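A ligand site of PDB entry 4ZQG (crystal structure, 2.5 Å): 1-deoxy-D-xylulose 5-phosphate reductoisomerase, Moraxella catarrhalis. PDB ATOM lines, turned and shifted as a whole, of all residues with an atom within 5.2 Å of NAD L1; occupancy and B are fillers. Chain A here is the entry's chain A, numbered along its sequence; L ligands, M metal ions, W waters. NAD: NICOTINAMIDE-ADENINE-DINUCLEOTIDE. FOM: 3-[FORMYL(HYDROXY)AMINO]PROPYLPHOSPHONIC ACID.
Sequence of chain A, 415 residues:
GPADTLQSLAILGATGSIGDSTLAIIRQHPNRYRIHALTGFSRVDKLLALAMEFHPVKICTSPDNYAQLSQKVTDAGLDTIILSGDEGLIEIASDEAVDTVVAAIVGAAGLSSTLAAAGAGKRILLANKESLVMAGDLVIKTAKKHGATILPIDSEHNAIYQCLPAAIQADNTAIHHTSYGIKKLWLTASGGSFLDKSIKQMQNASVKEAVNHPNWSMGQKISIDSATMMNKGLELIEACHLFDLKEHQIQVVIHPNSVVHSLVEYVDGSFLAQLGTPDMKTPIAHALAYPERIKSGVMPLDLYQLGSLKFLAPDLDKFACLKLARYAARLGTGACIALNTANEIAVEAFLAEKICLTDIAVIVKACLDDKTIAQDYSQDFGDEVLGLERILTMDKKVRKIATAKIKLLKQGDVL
The backbone carbonyl oxygen of Ala 127 lies close to an oxygen (O4D) of NAD L1. Ala 14 touches NAD L1 (N to O3B, 3.9 Å). Gly 40 touches NAD L1. Arg 43 touches NAD L1 (NH2 to C3B, 3.9 Å). O of Ala 104 touches C5D of NAD L1 (3.4 Å). Ile 105 touches NAD L1 (CA to O4B, 3.4 Å). N of Val 106 touches O4B of NAD L1, at 3.5 Å. CB of Ala 109 touches C6A of NAD L1 (3.5 Å). Asn 128 touches NAD L1 (CA to O3D, 3.2 Å). Lys 129 touches NAD L1. Asp 154 touches NAD L1. CB of Met 218 touches N7N of NAD L1 (3.4 Å). Ile 222 touches NAD L1. CG of Met 280 touches O7N of NAD L1 (3.2 Å). Hydrophobic or aromatic side chains that line NAD L1: Ile 18, Phe 41, Ile 105, Val 106, Ala 109, Ala 127, Met 218, Ile 222 and Met 280. The nearest printed residue that does not touch NAD L1 is Ser 217 (4.3 Å).
ND2 of Asn 128 sits at hydrogen-bond distance from OE1 of Glu 130 (3.1 Å). OE1 of Glu 130 lies within hydrogen-bond range of N of Gly 107 (3.4 Å). O of Ser 217 is in hydrogen-bond range of OG of Ser 17 (3.4 Å). The backbone NH (N) of Gly 13 is in hydrogen-bond range of the side-chain hydroxyl (OG1) of Thr 39, at 2.8 Å. The backbone carbonyl oxygen of Ile 105 sits at hydrogen-bond distance from the side-chain amide nitrogen of Asn 128 (2.9 Å). The side-chain amide nitrogen (ND2) of Asn 128 lies within hydrogen-bond range of the backbone carbonyl oxygen (O) of Gly 107. OD2 of Asp 154 is in salt-bridge range of NZ of Lys 129. The backbone NH (N) of Ala 14 sits at hydrogen-bond distance from the backbone carbonyl oxygen (O) of Thr 39 (2.8 Å).
An oxygen (O3D) of NAD L1 sits at hydrogen-bond distance from the side-chain carboxylate (OE1) of Glu 130 (2.6 Å). The backbone NH of Thr 15 lies within hydrogen-bond range of an oxygen (O3B) of NAD L1 (3.4 Å). OG1 of Thr 15 lies within hydrogen-bond range of O3B of NAD L1 (2.7 Å). The backbone NH of Phe 41 lies within hydrogen-bond range of an oxygen (O2B) of NAD L1, 2.8 Å away. The backbone NH (N) of Gly 219 lies within hydrogen-bond range of an oxygen (O1N) of NAD L1, at 2.8 Å. The backbone NH (N) of Ile 18 lies within hydrogen-bond range of an oxygen (O2N) of NAD L1 (3.0 Å). O2A of NAD L1 sits at hydrogen-bond distance from N of Ser 17 (3.0 Å). O of Gly 13 lies within hydrogen-bond range of O3B of NAD L1 (3.2 Å). The backbone NH (N) of Gly 16 sits at hydrogen-bond distance from an oxygen (O3B) of NAD L1 (3.2 Å). An oxygen (O1) of FOM L2 sits close to the backbone NH (N) of Ser 155, 3.3 Å away.
Water W2 lies within hydrogen-bond range of O2B of NAD L1 (2.8 Å), NE of Arg 43 (3.0 Å), N of Ser 42 (3.1 Å) and OG1 of Thr 15 (3.3 Å). Water W1 lies within hydrogen-bond range of the side-chain hydroxyl (OG1) of Thr 39 (2.7 Å), a nitrogen (N3A) of NAD L1 (3.3 Å) and the backbone NH (N) of Gly 40 (3.4 Å).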
ATOM      1  N   GLY A  13      12.116  -9.744 -16.238  1.00  0.00           N
ATOM      2  CA  GLY A  13      11.181 -10.758 -15.704  1.00  0.00           C
ATOM      3  C   GLY A  13      11.206 -11.994 -16.563  1.00  0.00           C
ATOM      4  O   GLY A  13      10.217 -12.660 -16.713  1.00  0.00           O
ATOM      5  N   ALA A  14      12.389 -12.338 -17.091  1.00  0.00           N
ATOM      6  CA  ALA A  14      12.579 -13.450 -18.055  1.00  0.00           C
ATOM      7  C   ALA A  14      12.315 -14.841 -17.567  1.00  0.00           C
ATOM      8  O   ALA A  14      12.211 -15.742 -18.376  1.00  0.00           O
ATOM      9  CB  ALA A  14      13.986 -13.402 -18.641  1.00  0.00           C
ATOM     10  N   THR A  15      12.219 -15.031 -16.258  1.00  0.00           N
ATOM     11  CA  THR A  15      12.095 -16.366 -15.653  1.00  0.00           C
ATOM     12  C   THR A  15      10.694 -16.742 -15.363  1.00  0.00           C
ATOM     13  O   THR A  15      10.429 -17.867 -15.035  1.00  0.00           O
ATOM     14  CB  THR A  15      12.879 -16.482 -14.318  1.00  0.00           C
ATOM     15  OG1 THR A  15      12.514 -15.408 -13.424  1.00  0.00           O
ATOM     16  CG2 THR A  15      14.371 -16.435 -14.568  1.00  0.00           C
ATOM     17  N   GLY A  16       9.763 -15.806 -15.455  1.00  0.00           N
ATOM     18  CA  GLY A  16       8.376 -16.117 -15.141  1.00  0.00           C
ATOM     19  C   GLY A  16       7.598 -16.626 -16.345  1.00  0.00           C
ATOM     20  O   GLY A  16       8.168 -16.963 -17.398  1.00  0.00           O
ATOM     21  N   SER A  17       6.281 -16.656 -16.188  1.00  0.00           N
ATOM     22  CA  SER A  17       5.372 -17.223 -17.173  1.00  0.00           C
ATOM     23  C   SER A  17       5.479 -16.490 -18.508  1.00  0.00           C
ATOM     24  O   SER A  17       5.713 -17.082 -19.573  1.00  0.00           O
ATOM     25  CB  SER A  17       3.964 -17.092 -16.604  1.00  0.00           C
ATOM     26  OG  SER A  17       3.122 -18.033 -17.187  1.00  0.00           O
ATOM     27  N   ILE A  18       5.363 -15.161 -18.411  1.00  0.00           N
ATOM     28  CA  ILE A  18       5.448 -14.296 -19.553  1.00  0.00           C
ATOM     29  C   ILE A  18       6.820 -14.495 -20.212  1.00  0.00           C
ATOM     30  O   ILE A  18       6.940 -14.647 -21.429  1.00  0.00           O
ATOM     31  CB  ILE A  18       5.157 -12.816 -19.143  1.00  0.00           C
ATOM     32  CG1 ILE A  18       3.708 -12.640 -18.787  1.00  0.00           C
ATOM     33  CG2 ILE A  18       5.516 -11.836 -20.232  1.00  0.00           C
ATOM     34  CD1 ILE A  18       2.726 -12.800 -19.947  1.00  0.00           C
ATOM     35  N   GLY A  19       7.859 -14.527 -19.398  1.00  0.00           N
ATOM     36  CA  GLY A  19       9.197 -14.735 -19.906  1.00  0.00           C
ATOM     37  C   GLY A  19       9.364 -16.022 -20.652  1.00  0.00           C
ATOM     38  O   GLY A  19       9.955 -16.029 -21.721  1.00  0.00           O
ATOM     39  N   THR A  39      16.437 -10.831 -16.878  1.00  0.00           N
ATOM     40  CA  THR A  39      16.451 -10.589 -15.458  1.00  0.00           C
ATOM     41  C   THR A  39      15.560 -11.536 -14.739  1.00  0.00           C
ATOM     42  O   THR A  39      14.554 -11.972 -15.278  1.00  0.00           O
ATOM     43  CB  THR A  39      15.954  -9.196 -15.082  1.00  0.00           C
ATOM     44  OG1 THR A  39      14.512  -9.171 -14.936  1.00  0.00           O
ATOM     45  CG2 THR A  39      16.466  -8.129 -16.071  1.00  0.00           C
ATOM     46  N   GLY A  40      15.922 -11.843 -13.500  1.00  0.00           N
ATOM     47  CA  GLY A  40      15.189 -12.802 -12.681  1.00  0.00           C
ATOM     48  C   GLY A  40      15.441 -12.546 -11.222  1.00  0.00           C
ATOM     49  O   GLY A  40      16.547 -12.250 -10.839  1.00  0.00           O
ATOM     50  N   PHE A  41      14.435 -12.650 -10.363  1.00  0.00           N
ATOM     51  CA  PHE A  41      14.609 -12.248  -8.986  1.00  0.00           C
ATOM     52  C   PHE A  41      15.127 -13.417  -8.173  1.00  0.00           C
ATOM     53  O   PHE A  41      16.194 -13.314  -7.615  1.00  0.00           O
ATOM     54  CB  PHE A  41      13.281 -11.693  -8.418  1.00  0.00           C
ATOM     55  CG  PHE A  41      13.430 -10.936  -7.116  1.00  0.00           C
ATOM     56  CD1 PHE A  41      12.978 -11.496  -5.918  1.00  0.00           C
ATOM     57  CD2 PHE A  41      13.984  -9.648  -7.081  1.00  0.00           C
ATOM     58  CE1 PHE A  41      13.088 -10.799  -4.718  1.00  0.00           C
ATOM     59  CE2 PHE A  41      14.092  -8.943  -5.892  1.00  0.00           C
ATOM     60  CZ  PHE A  41      13.629  -9.520  -4.721  1.00  0.00           C
ATOM     61  N   SER A  42      14.389 -14.522  -8.143  1.00  0.00           N
ATOM     62  CA  SER A  42      14.693 -15.631  -7.245  1.00  0.00           C
ATOM     63  C   SER A  42      15.369 -16.837  -7.895  1.00  0.00           C
ATOM     64  O   SER A  42      16.166 -17.498  -7.259  1.00  0.00           O
ATOM     65  CB  SER A  42      13.410 -16.132  -6.571  1.00  0.00           C
ATOM     66  OG  SER A  42      13.153 -15.401  -5.387  1.00  0.00           O
ATOM     67  N   ARG A  43      15.000 -17.153  -9.139  1.00  0.00           N
ATOM     68  CA  ARG A  43      15.357 -18.446  -9.709  1.00  0.00           C
ATOM     69  C   ARG A  43      16.712 -18.355 -10.401  1.00  0.00           C
ATOM     70  O   ARG A  43      16.810 -18.280 -11.641  1.00  0.00           O
ATOM     71  CB  ARG A  43      14.249 -18.937 -10.644  1.00  0.00           C
ATOM     72  CG  ARG A  43      13.128 -19.688  -9.936  1.00  0.00           C
ATOM     73  CD  ARG A  43      11.833 -19.649 -10.717  1.00  0.00           C
ATOM     74  NE  ARG A  43      11.226 -18.319 -10.620  1.00  0.00           N
ATOM     75  CZ  ARG A  43      10.027 -17.984 -11.100  1.00  0.00           C
ATOM     76  NH1 ARG A  43       9.289 -18.896 -11.741  1.00  0.00           N
ATOM     77  NH2 ARG A  43       9.547 -16.737 -10.950  1.00  0.00           N
ATOM     78  N   LEU A  89      17.972  -3.011 -12.972  1.00  0.00           N
ATOM     79  CA  LEU A  89      16.856  -2.981 -13.864  1.00  0.00           C
ATOM     80  C   LEU A  89      16.789  -1.651 -14.626  1.00  0.00           C
ATOM     81  O   LEU A  89      16.589  -1.618 -15.830  1.00  0.00           O
ATOM     82  CB  LEU A  89      15.558  -3.213 -13.090  1.00  0.00           C
ATOM     83  CG  LEU A  89      15.495  -4.486 -12.240  1.00  0.00           C
ATOM     84  CD1 LEU A  89      14.177  -4.598 -11.492  1.00  0.00           C
ATOM     85  CD2 LEU A  89      15.727  -5.690 -13.111  1.00  0.00           C
ATOM     86  N   ALA A 104       8.058  -7.454 -17.857  1.00  0.00           N
ATOM     87  CA  ALA A 104       7.281  -8.561 -17.268  1.00  0.00           C
ATOM     88  C   ALA A 104       7.582  -8.840 -15.828  1.00  0.00           C
ATOM     89  O   ALA A 104       7.354  -9.945 -15.391  1.00  0.00           O
ATOM     90  CB  ALA A 104       7.429  -9.857 -18.068  1.00  0.00           C
ATOM     91  N   ILE A 105       8.053  -7.830 -15.098  1.00  0.00           N
ATOM     92  CA  ILE A 105       8.207  -7.941 -13.664  1.00  0.00           C
ATOM     93  C   ILE A 105       6.828  -7.836 -13.085  1.00  0.00           C
ATOM     94  O   ILE A 105       6.129  -6.967 -13.455  1.00  0.00           O
ATOM     95  CB  ILE A 105       8.967  -6.745 -13.043  1.00  0.00           C
ATOM     96  CG1 ILE A 105      10.394  -6.542 -13.616  1.00  0.00           C
ATOM     97  CG2 ILE A 105       9.044  -6.906 -11.529  1.00  0.00           C
ATOM     98  CD1 ILE A 105      11.059  -7.789 -14.073  1.00  0.00           C
ATOM     99  N   VAL A 106       6.445  -8.683 -12.163  1.00  0.00           N
ATOM    100  CA  VAL A 106       5.112  -8.585 -11.556  1.00  0.00           C
ATOM    101  C   VAL A 106       5.042  -7.486 -10.491  1.00  0.00           C
ATOM    102  O   VAL A 106       6.009  -7.194  -9.796  1.00  0.00           O
ATOM    103  CB  VAL A 106       4.638  -9.926 -10.948  1.00  0.00           C
ATOM    104  CG1 VAL A 106       5.502 -10.325  -9.764  1.00  0.00           C
ATOM    105  CG2 VAL A 106       3.193  -9.843 -10.499  1.00  0.00           C
ATOM    106  N   GLY A 107       3.872  -6.863 -10.387  1.00  0.00           N
ATOM    107  CA  GLY A 107       3.534  -5.929  -9.316  1.00  0.00           C
ATOM    108  C   GLY A 107       4.199  -4.574  -9.446  1.00  0.00           C
ATOM    109  O   GLY A 107       4.642  -4.179 -10.527  1.00  0.00           O
ATOM    110  N   ALA A 109       6.965  -3.823  -8.140  1.00  0.00           N
ATOM    111  CA  ALA A 109       8.392  -3.995  -8.356  1.00  0.00           C
ATOM    112  C   ALA A 109       8.829  -3.648  -9.792  1.00  0.00           C
ATOM    113  O   ALA A 109       9.978  -3.365 -10.022  1.00  0.00           O
ATOM    114  CB  ALA A 109       8.795  -5.412  -7.991  1.00  0.00           C
ATOM    115  N   ALA A 127       3.585  -6.182 -20.122  1.00  0.00           N
ATOM    116  CA  ALA A 127       2.788  -7.243 -19.539  1.00  0.00           C
ATOM    117  C   ALA A 127       2.378  -6.712 -18.210  1.00  0.00           C
ATOM    118  O   ALA A 127       1.218  -6.738 -17.819  1.00  0.00           O
ATOM    119  CB  ALA A 127       3.623  -8.503 -19.366  1.00  0.00           C
ATOM    120  N   ASN A 128       3.378  -6.250 -17.512  1.00  0.00           N
ATOM    121  CA  ASN A 128       3.291  -5.677 -16.190  1.00  0.00           C
ATOM    122  C   ASN A 128       2.261  -4.536 -16.073  1.00  0.00           C
ATOM    123  O   ASN A 128       2.583  -3.339 -16.270  1.00  0.00           O
ATOM    124  CB  ASN A 128       4.693  -5.184 -15.859  1.00  0.00           C
ATOM    125  CG  ASN A 128       4.749  -4.457 -14.581  1.00  0.00           C
ATOM    126  OD1 ASN A 128       5.413  -3.430 -14.489  1.00  0.00           O
ATOM    127  ND2 ASN A 128       4.055  -4.978 -13.567  1.00  0.00           N
ATOM    128  N   LYS A 129       1.052  -4.913 -15.718  1.00  0.00           N
ATOM    129  CA  LYS A 129      -0.120  -3.987 -15.695  1.00  0.00           C
ATOM    130  C   LYS A 129      -0.142  -3.123 -14.426  1.00  0.00           C
ATOM    131  O   LYS A 129      -0.615  -1.984 -14.458  1.00  0.00           O
ATOM    132  CB  LYS A 129      -1.451  -4.753 -15.811  1.00  0.00           C
ATOM    133  CG  LYS A 129      -1.688  -5.706 -14.629  1.00  0.00           C
ATOM    134  CD  LYS A 129      -2.899  -6.578 -14.847  1.00  0.00           C
ATOM    135  CE  LYS A 129      -2.760  -7.426 -16.081  1.00  0.00           C
ATOM    136  NZ  LYS A 129      -3.708  -8.572 -16.018  1.00  0.00           N
ATOM    137  N   GLU A 130       0.387  -3.652 -13.319  1.00  0.00           N
ATOM    138  CA  GLU A 130       0.535  -2.869 -12.121  1.00  0.00           C
ATOM    139  C   GLU A 130       1.331  -1.567 -12.364  1.00  0.00           C
ATOM    140  O   GLU A 130       1.099  -0.571 -11.705  1.00  0.00           O
ATOM    141  CB  GLU A 130       1.130  -3.728 -11.002  1.00  0.00           C
ATOM    142  CG  GLU A 130       0.304  -4.984 -10.660  1.00  0.00           C
ATOM    143  CD  GLU A 130       0.674  -6.251 -11.477  1.00  0.00           C
ATOM    144  OE1 GLU A 130       1.313  -6.135 -12.553  1.00  0.00           O
ATOM    145  OE2 GLU A 130       0.305  -7.391 -11.072  1.00  0.00           O
ATOM    146  N   ASP A 154      -0.644  -7.773 -22.567  1.00  0.00           N
ATOM    147  CA  ASP A 154      -1.818  -8.277 -21.921  1.00  0.00           C
ATOM    148  C   ASP A 154      -2.892  -8.626 -23.005  1.00  0.00           C
ATOM    149  O   ASP A 154      -3.119  -7.850 -23.948  1.00  0.00           O
ATOM    150  CB  ASP A 154      -2.340  -7.264 -20.890  1.00  0.00           C
ATOM    151  CG  ASP A 154      -3.183  -7.941 -19.825  1.00  0.00           C
ATOM    152  OD1 ASP A 154      -3.534  -9.091 -20.087  1.00  0.00           O
ATOM    153  OD2 ASP A 154      -3.454  -7.366 -18.754  1.00  0.00           O
ATOM    154  N   SER A 155      -3.503  -9.786 -22.886  1.00  0.00           N
ATOM    155  CA  SER A 155      -4.382 -10.342 -23.923  1.00  0.00           C
ATOM    156  C   SER A 155      -5.497  -9.393 -24.362  1.00  0.00           C
ATOM    157  O   SER A 155      -5.592  -8.998 -25.537  1.00  0.00           O
ATOM    158  CB  SER A 155      -5.018 -11.648 -23.434  1.00  0.00           C
ATOM    159  OG  SER A 155      -5.466 -12.437 -24.518  1.00  0.00           O
ATOM    160  N   TRP A 216      -6.014 -20.924 -18.557  1.00  0.00           N
ATOM    161  CA  TRP A 216      -4.734 -20.221 -18.629  1.00  0.00           C
ATOM    162  C   TRP A 216      -3.758 -20.815 -17.615  1.00  0.00           C
ATOM    163  O   TRP A 216      -4.184 -21.232 -16.545  1.00  0.00           O
ATOM    164  CB  TRP A 216      -4.934 -18.762 -18.229  1.00  0.00           C
ATOM    165  CG  TRP A 216      -5.604 -17.895 -19.166  1.00  0.00           C
ATOM    166  CD1 TRP A 216      -6.878 -17.410 -19.062  1.00  0.00           C
ATOM    167  CD2 TRP A 216      -5.043 -17.314 -20.333  1.00  0.00           C
ATOM    168  NE1 TRP A 216      -7.139 -16.560 -20.112  1.00  0.00           N
ATOM    169  CE2 TRP A 216      -6.034 -16.489 -20.905  1.00  0.00           C
ATOM    170  CE3 TRP A 216      -3.793 -17.407 -20.968  1.00  0.00           C
ATOM    171  CZ2 TRP A 216      -5.831 -15.779 -22.070  1.00  0.00           C
ATOM    172  CZ3 TRP A 216      -3.598 -16.708 -22.129  1.00  0.00           C
ATOM    173  CH2 TRP A 216      -4.602 -15.885 -22.673  1.00  0.00           C
ATOM    174  N   SER A 217      -2.476 -20.825 -17.965  1.00  0.00           N
ATOM    175  CA  SER A 217      -1.382 -21.072 -17.023  1.00  0.00           C
ATOM    176  C   SER A 217      -0.571 -19.811 -16.851  1.00  0.00           C
ATOM    177  O   SER A 217      -0.027 -19.283 -17.823  1.00  0.00           O
ATOM    178  CB  SER A 217      -0.456 -22.161 -17.533  1.00  0.00           C
ATOM    179  OG  SER A 217      -0.797 -23.387 -16.940  1.00  0.00           O
ATOM    180  N   MET A 218      -0.493 -19.302 -15.623  1.00  0.00           N
ATOM    181  CA  MET A 218       0.092 -17.993 -15.380  1.00  0.00           C
ATOM    182  C   MET A 218       0.823 -17.983 -14.068  1.00  0.00           C
ATOM    183  O   MET A 218       0.859 -18.989 -13.348  1.00  0.00           O
ATOM    184  CB  MET A 218      -1.008 -16.942 -15.360  1.00  0.00           C
ATOM    185  CG  MET A 218      -1.957 -17.016 -16.539  1.00  0.00           C
ATOM    186  SD  MET A 218      -3.369 -15.925 -16.293  1.00  0.00           S
ATOM    187  CE  MET A 218      -4.399 -16.913 -15.201  1.00  0.00           C
ATOM    188  N   GLY A 219       1.415 -16.829 -13.732  1.00  0.00           N
ATOM    189  CA  GLY A 219       2.002 -16.635 -12.415  1.00  0.00           C
ATOM    190  C   GLY A 219       0.928 -16.779 -11.339  1.00  0.00           C
ATOM    191  O   GLY A 219      -0.271 -16.901 -11.624  1.00  0.00           O
ATOM    192  N   GLN A 220       1.370 -16.764 -10.092  1.00  0.00           N
ATOM    193  CA  GLN A 220       0.487 -16.962  -8.960  1.00  0.00           C
ATOM    194  C   GLN A 220      -0.454 -15.797  -8.709  1.00  0.00           C
ATOM    195  O   GLN A 220      -1.632 -15.986  -8.320  1.00  0.00           O
ATOM    196  CB  GLN A 220       1.325 -17.162  -7.713  1.00  0.00           C
ATOM    197  CG  GLN A 220       1.954 -18.539  -7.586  1.00  0.00           C
ATOM    198  CD  GLN A 220       2.420 -18.758  -6.164  1.00  0.00           C
ATOM    199  OE1 GLN A 220       3.409 -18.141  -5.716  1.00  0.00           O
ATOM    200  NE2 GLN A 220       1.673 -19.576  -5.411  1.00  0.00           N
ATOM    201  N   ILE A 222      -1.598 -12.901 -10.740  1.00  0.00           N
ATOM    202  CA  ILE A 222      -2.587 -12.784 -11.779  1.00  0.00           C
ATOM    203  C   ILE A 222      -3.540 -13.968 -11.671  1.00  0.00           C
ATOM    204  O   ILE A 222      -4.722 -13.826 -11.823  1.00  0.00           O
ATOM    205  CB  ILE A 222      -1.953 -12.617 -13.193  1.00  0.00           C
ATOM    206  CG1 ILE A 222      -2.952 -11.963 -14.134  1.00  0.00           C
ATOM    207  CG2 ILE A 222      -1.521 -13.919 -13.805  1.00  0.00           C
ATOM    208  CD1 ILE A 222      -2.404 -11.606 -15.503  1.00  0.00           C
ATOM    209  N   MET A 280      -0.587 -16.872 -24.358  1.00  0.00           N
ATOM    210  CA  MET A 280       0.039 -15.560 -24.455  1.00  0.00           C
ATOM    211  C   MET A 280       1.076 -15.414 -25.556  1.00  0.00           C
ATOM    212  O   MET A 280       1.547 -14.327 -25.786  1.00  0.00           O
ATOM    213  CB  MET A 280       0.700 -15.187 -23.131  1.00  0.00           C
ATOM    214  CG  MET A 280      -0.278 -14.937 -21.994  1.00  0.00           C
ATOM    215  SD  MET A 280      -1.487 -13.640 -22.303  1.00  0.00           S
ATOM    216  CE  MET A 280      -0.468 -12.189 -22.525  1.00  0.00           C
HETATM  217  PA  NAD L   1       5.517 -14.490 -12.632  1.00  0.00           P
HETATM  218  O1A NAD L   1       5.180 -14.430 -11.179  1.00  0.00           O
HETATM  219  O2A NAD L   1       5.407 -15.787 -13.403  1.00  0.00           O
HETATM  220  O5B NAD L   1       6.956 -13.822 -12.942  1.00  0.00           O
HETATM  221  C5B NAD L   1       7.341 -12.538 -12.500  1.00  0.00           C
HETATM  222  C4B NAD L   1       8.764 -12.190 -12.991  1.00  0.00           C
HETATM  223  O4B NAD L   1       9.145 -10.964 -12.334  1.00  0.00           O
HETATM  224  C3B NAD L   1       9.813 -13.251 -12.655  1.00  0.00           C
HETATM  225  O3B NAD L   1      10.800 -13.376 -13.683  1.00  0.00           O
HETATM  226  C2B NAD L   1      10.454 -12.710 -11.377  1.00  0.00           C
HETATM  227  O2B NAD L   1      11.850 -12.976 -11.284  1.00  0.00           O
HETATM  228  C1B NAD L   1      10.239 -11.205 -11.441  1.00  0.00           C
HETATM  229  N9A NAD L   1       9.991 -10.629 -10.085  1.00  0.00           N
HETATM  230  C8A NAD L   1       9.096 -11.093  -9.185  1.00  0.00           C
HETATM  231  N7A NAD L   1       9.123 -10.356  -8.050  1.00  0.00           N
HETATM  232  C5A NAD L   1      10.046  -9.405  -8.196  1.00  0.00           C
HETATM  233  C6A NAD L   1      10.547  -8.320  -7.326  1.00  0.00           C
HETATM  234  N6A NAD L   1      10.025  -8.133  -6.072  1.00  0.00           N
HETATM  235  N1A NAD L   1      11.522  -7.559  -7.860  1.00  0.00           N
HETATM  236  C2A NAD L   1      12.044  -7.779  -9.101  1.00  0.00           C
HETATM  237  N3A NAD L   1      11.645  -8.752  -9.946  1.00  0.00           N
HETATM  238  C4A NAD L   1      10.638  -9.583  -9.540  1.00  0.00           C
HETATM  239  O3  NAD L   1       4.589 -13.374 -13.335  1.00  0.00           O
HETATM  240  PN  NAD L   1       3.707 -13.455 -14.676  1.00  0.00           P
HETATM  241  O1N NAD L   1       2.499 -14.299 -14.308  1.00  0.00           O
HETATM  242  O2N NAD L   1       4.640 -13.730 -15.828  1.00  0.00           O
HETATM  243  O5D NAD L   1       3.272 -11.909 -14.719  1.00  0.00           O
HETATM  244  C5D NAD L   1       4.126 -10.900 -15.245  1.00  0.00           C
HETATM  245  C4D NAD L   1       3.328  -9.614 -15.498  1.00  0.00           C
HETATM  246  O4D NAD L   1       2.574  -9.699 -16.716  1.00  0.00           O
HETATM  247  C3D NAD L   1       2.338  -9.361 -14.381  1.00  0.00           C
HETATM  248  O3D NAD L   1       2.260  -7.957 -14.189  1.00  0.00           O
HETATM  249  C2D NAD L   1       1.043  -9.951 -14.883  1.00  0.00           C
HETATM  250  O2D NAD L   1      -0.093  -9.350 -14.244  1.00  0.00           O
HETATM  251  C1D NAD L   1       1.167  -9.687 -16.386  1.00  0.00           C
HETATM  252  N1N NAD L   1       0.434 -10.679 -17.197  1.00  0.00           N
HETATM  253  C2N NAD L   1       0.765 -11.998 -17.157  1.00  0.00           C
HETATM  254  C3N NAD L   1       0.042 -12.946 -17.906  1.00  0.00           C
HETATM  255  C7N NAD L   1       0.382 -14.411 -17.908  1.00  0.00           C
HETATM  256  O7N NAD L   1      -0.066 -15.139 -18.775  1.00  0.00           O
HETATM  257  N7N NAD L   1       1.199 -14.918 -16.979  1.00  0.00           N
HETATM  258  C4N NAD L   1      -1.014 -12.513 -18.695  1.00  0.00           C
HETATM  259  C5N NAD L   1      -1.301 -11.168 -18.720  1.00  0.00           C
HETATM  260  C6N NAD L   1      -0.574 -10.258 -17.971  1.00  0.00           C
HETATM  261  O2  FOM L   2      -5.160 -11.648 -17.875  1.00  0.00           O
HETATM  262  N1  FOM L   2      -5.152 -12.781 -18.677  1.00  0.00           N
HETATM  263  C1  FOM L   2      -4.754 -12.734 -19.880  1.00  0.00           C
HETATM  264  O1  FOM L   2      -4.382 -11.690 -20.386  1.00  0.00           O
HETATM  265  C2  FOM L   2      -5.691 -13.976 -18.040  1.00  0.00           C
HETATM  266  C3  FOM L   2      -7.126 -13.486 -17.788  1.00  0.00           C
HETATM  267  C4  FOM L   2      -7.900 -14.443 -16.931  1.00  0.00           C
HETATM  268  PA1 FOM L   2      -9.463 -13.633 -16.646  1.00  0.00           P
HETATM  269  OP1 FOM L   2     -10.186 -13.518 -18.067  1.00  0.00           O
HETATM  270  OP2 FOM L   2      -9.222 -12.242 -16.271  1.00  0.00           O
HETATM  271  OP3 FOM L   2     -10.427 -14.352 -15.553  1.00  0.00           O
HETATM  272 MG    MG M   1      -5.230 -10.024 -19.256  1.00  0.00          MG
HETATM  273  O   HOH W   1      13.419  -9.834 -12.505  1.00  0.00           O
HETATM  274  O   HOH W   2      12.179 -15.550 -10.117  1.00  0.00           O
HETATM  275  O   HOH W   3       7.362 -13.469 -16.472  1.00  0.00           O
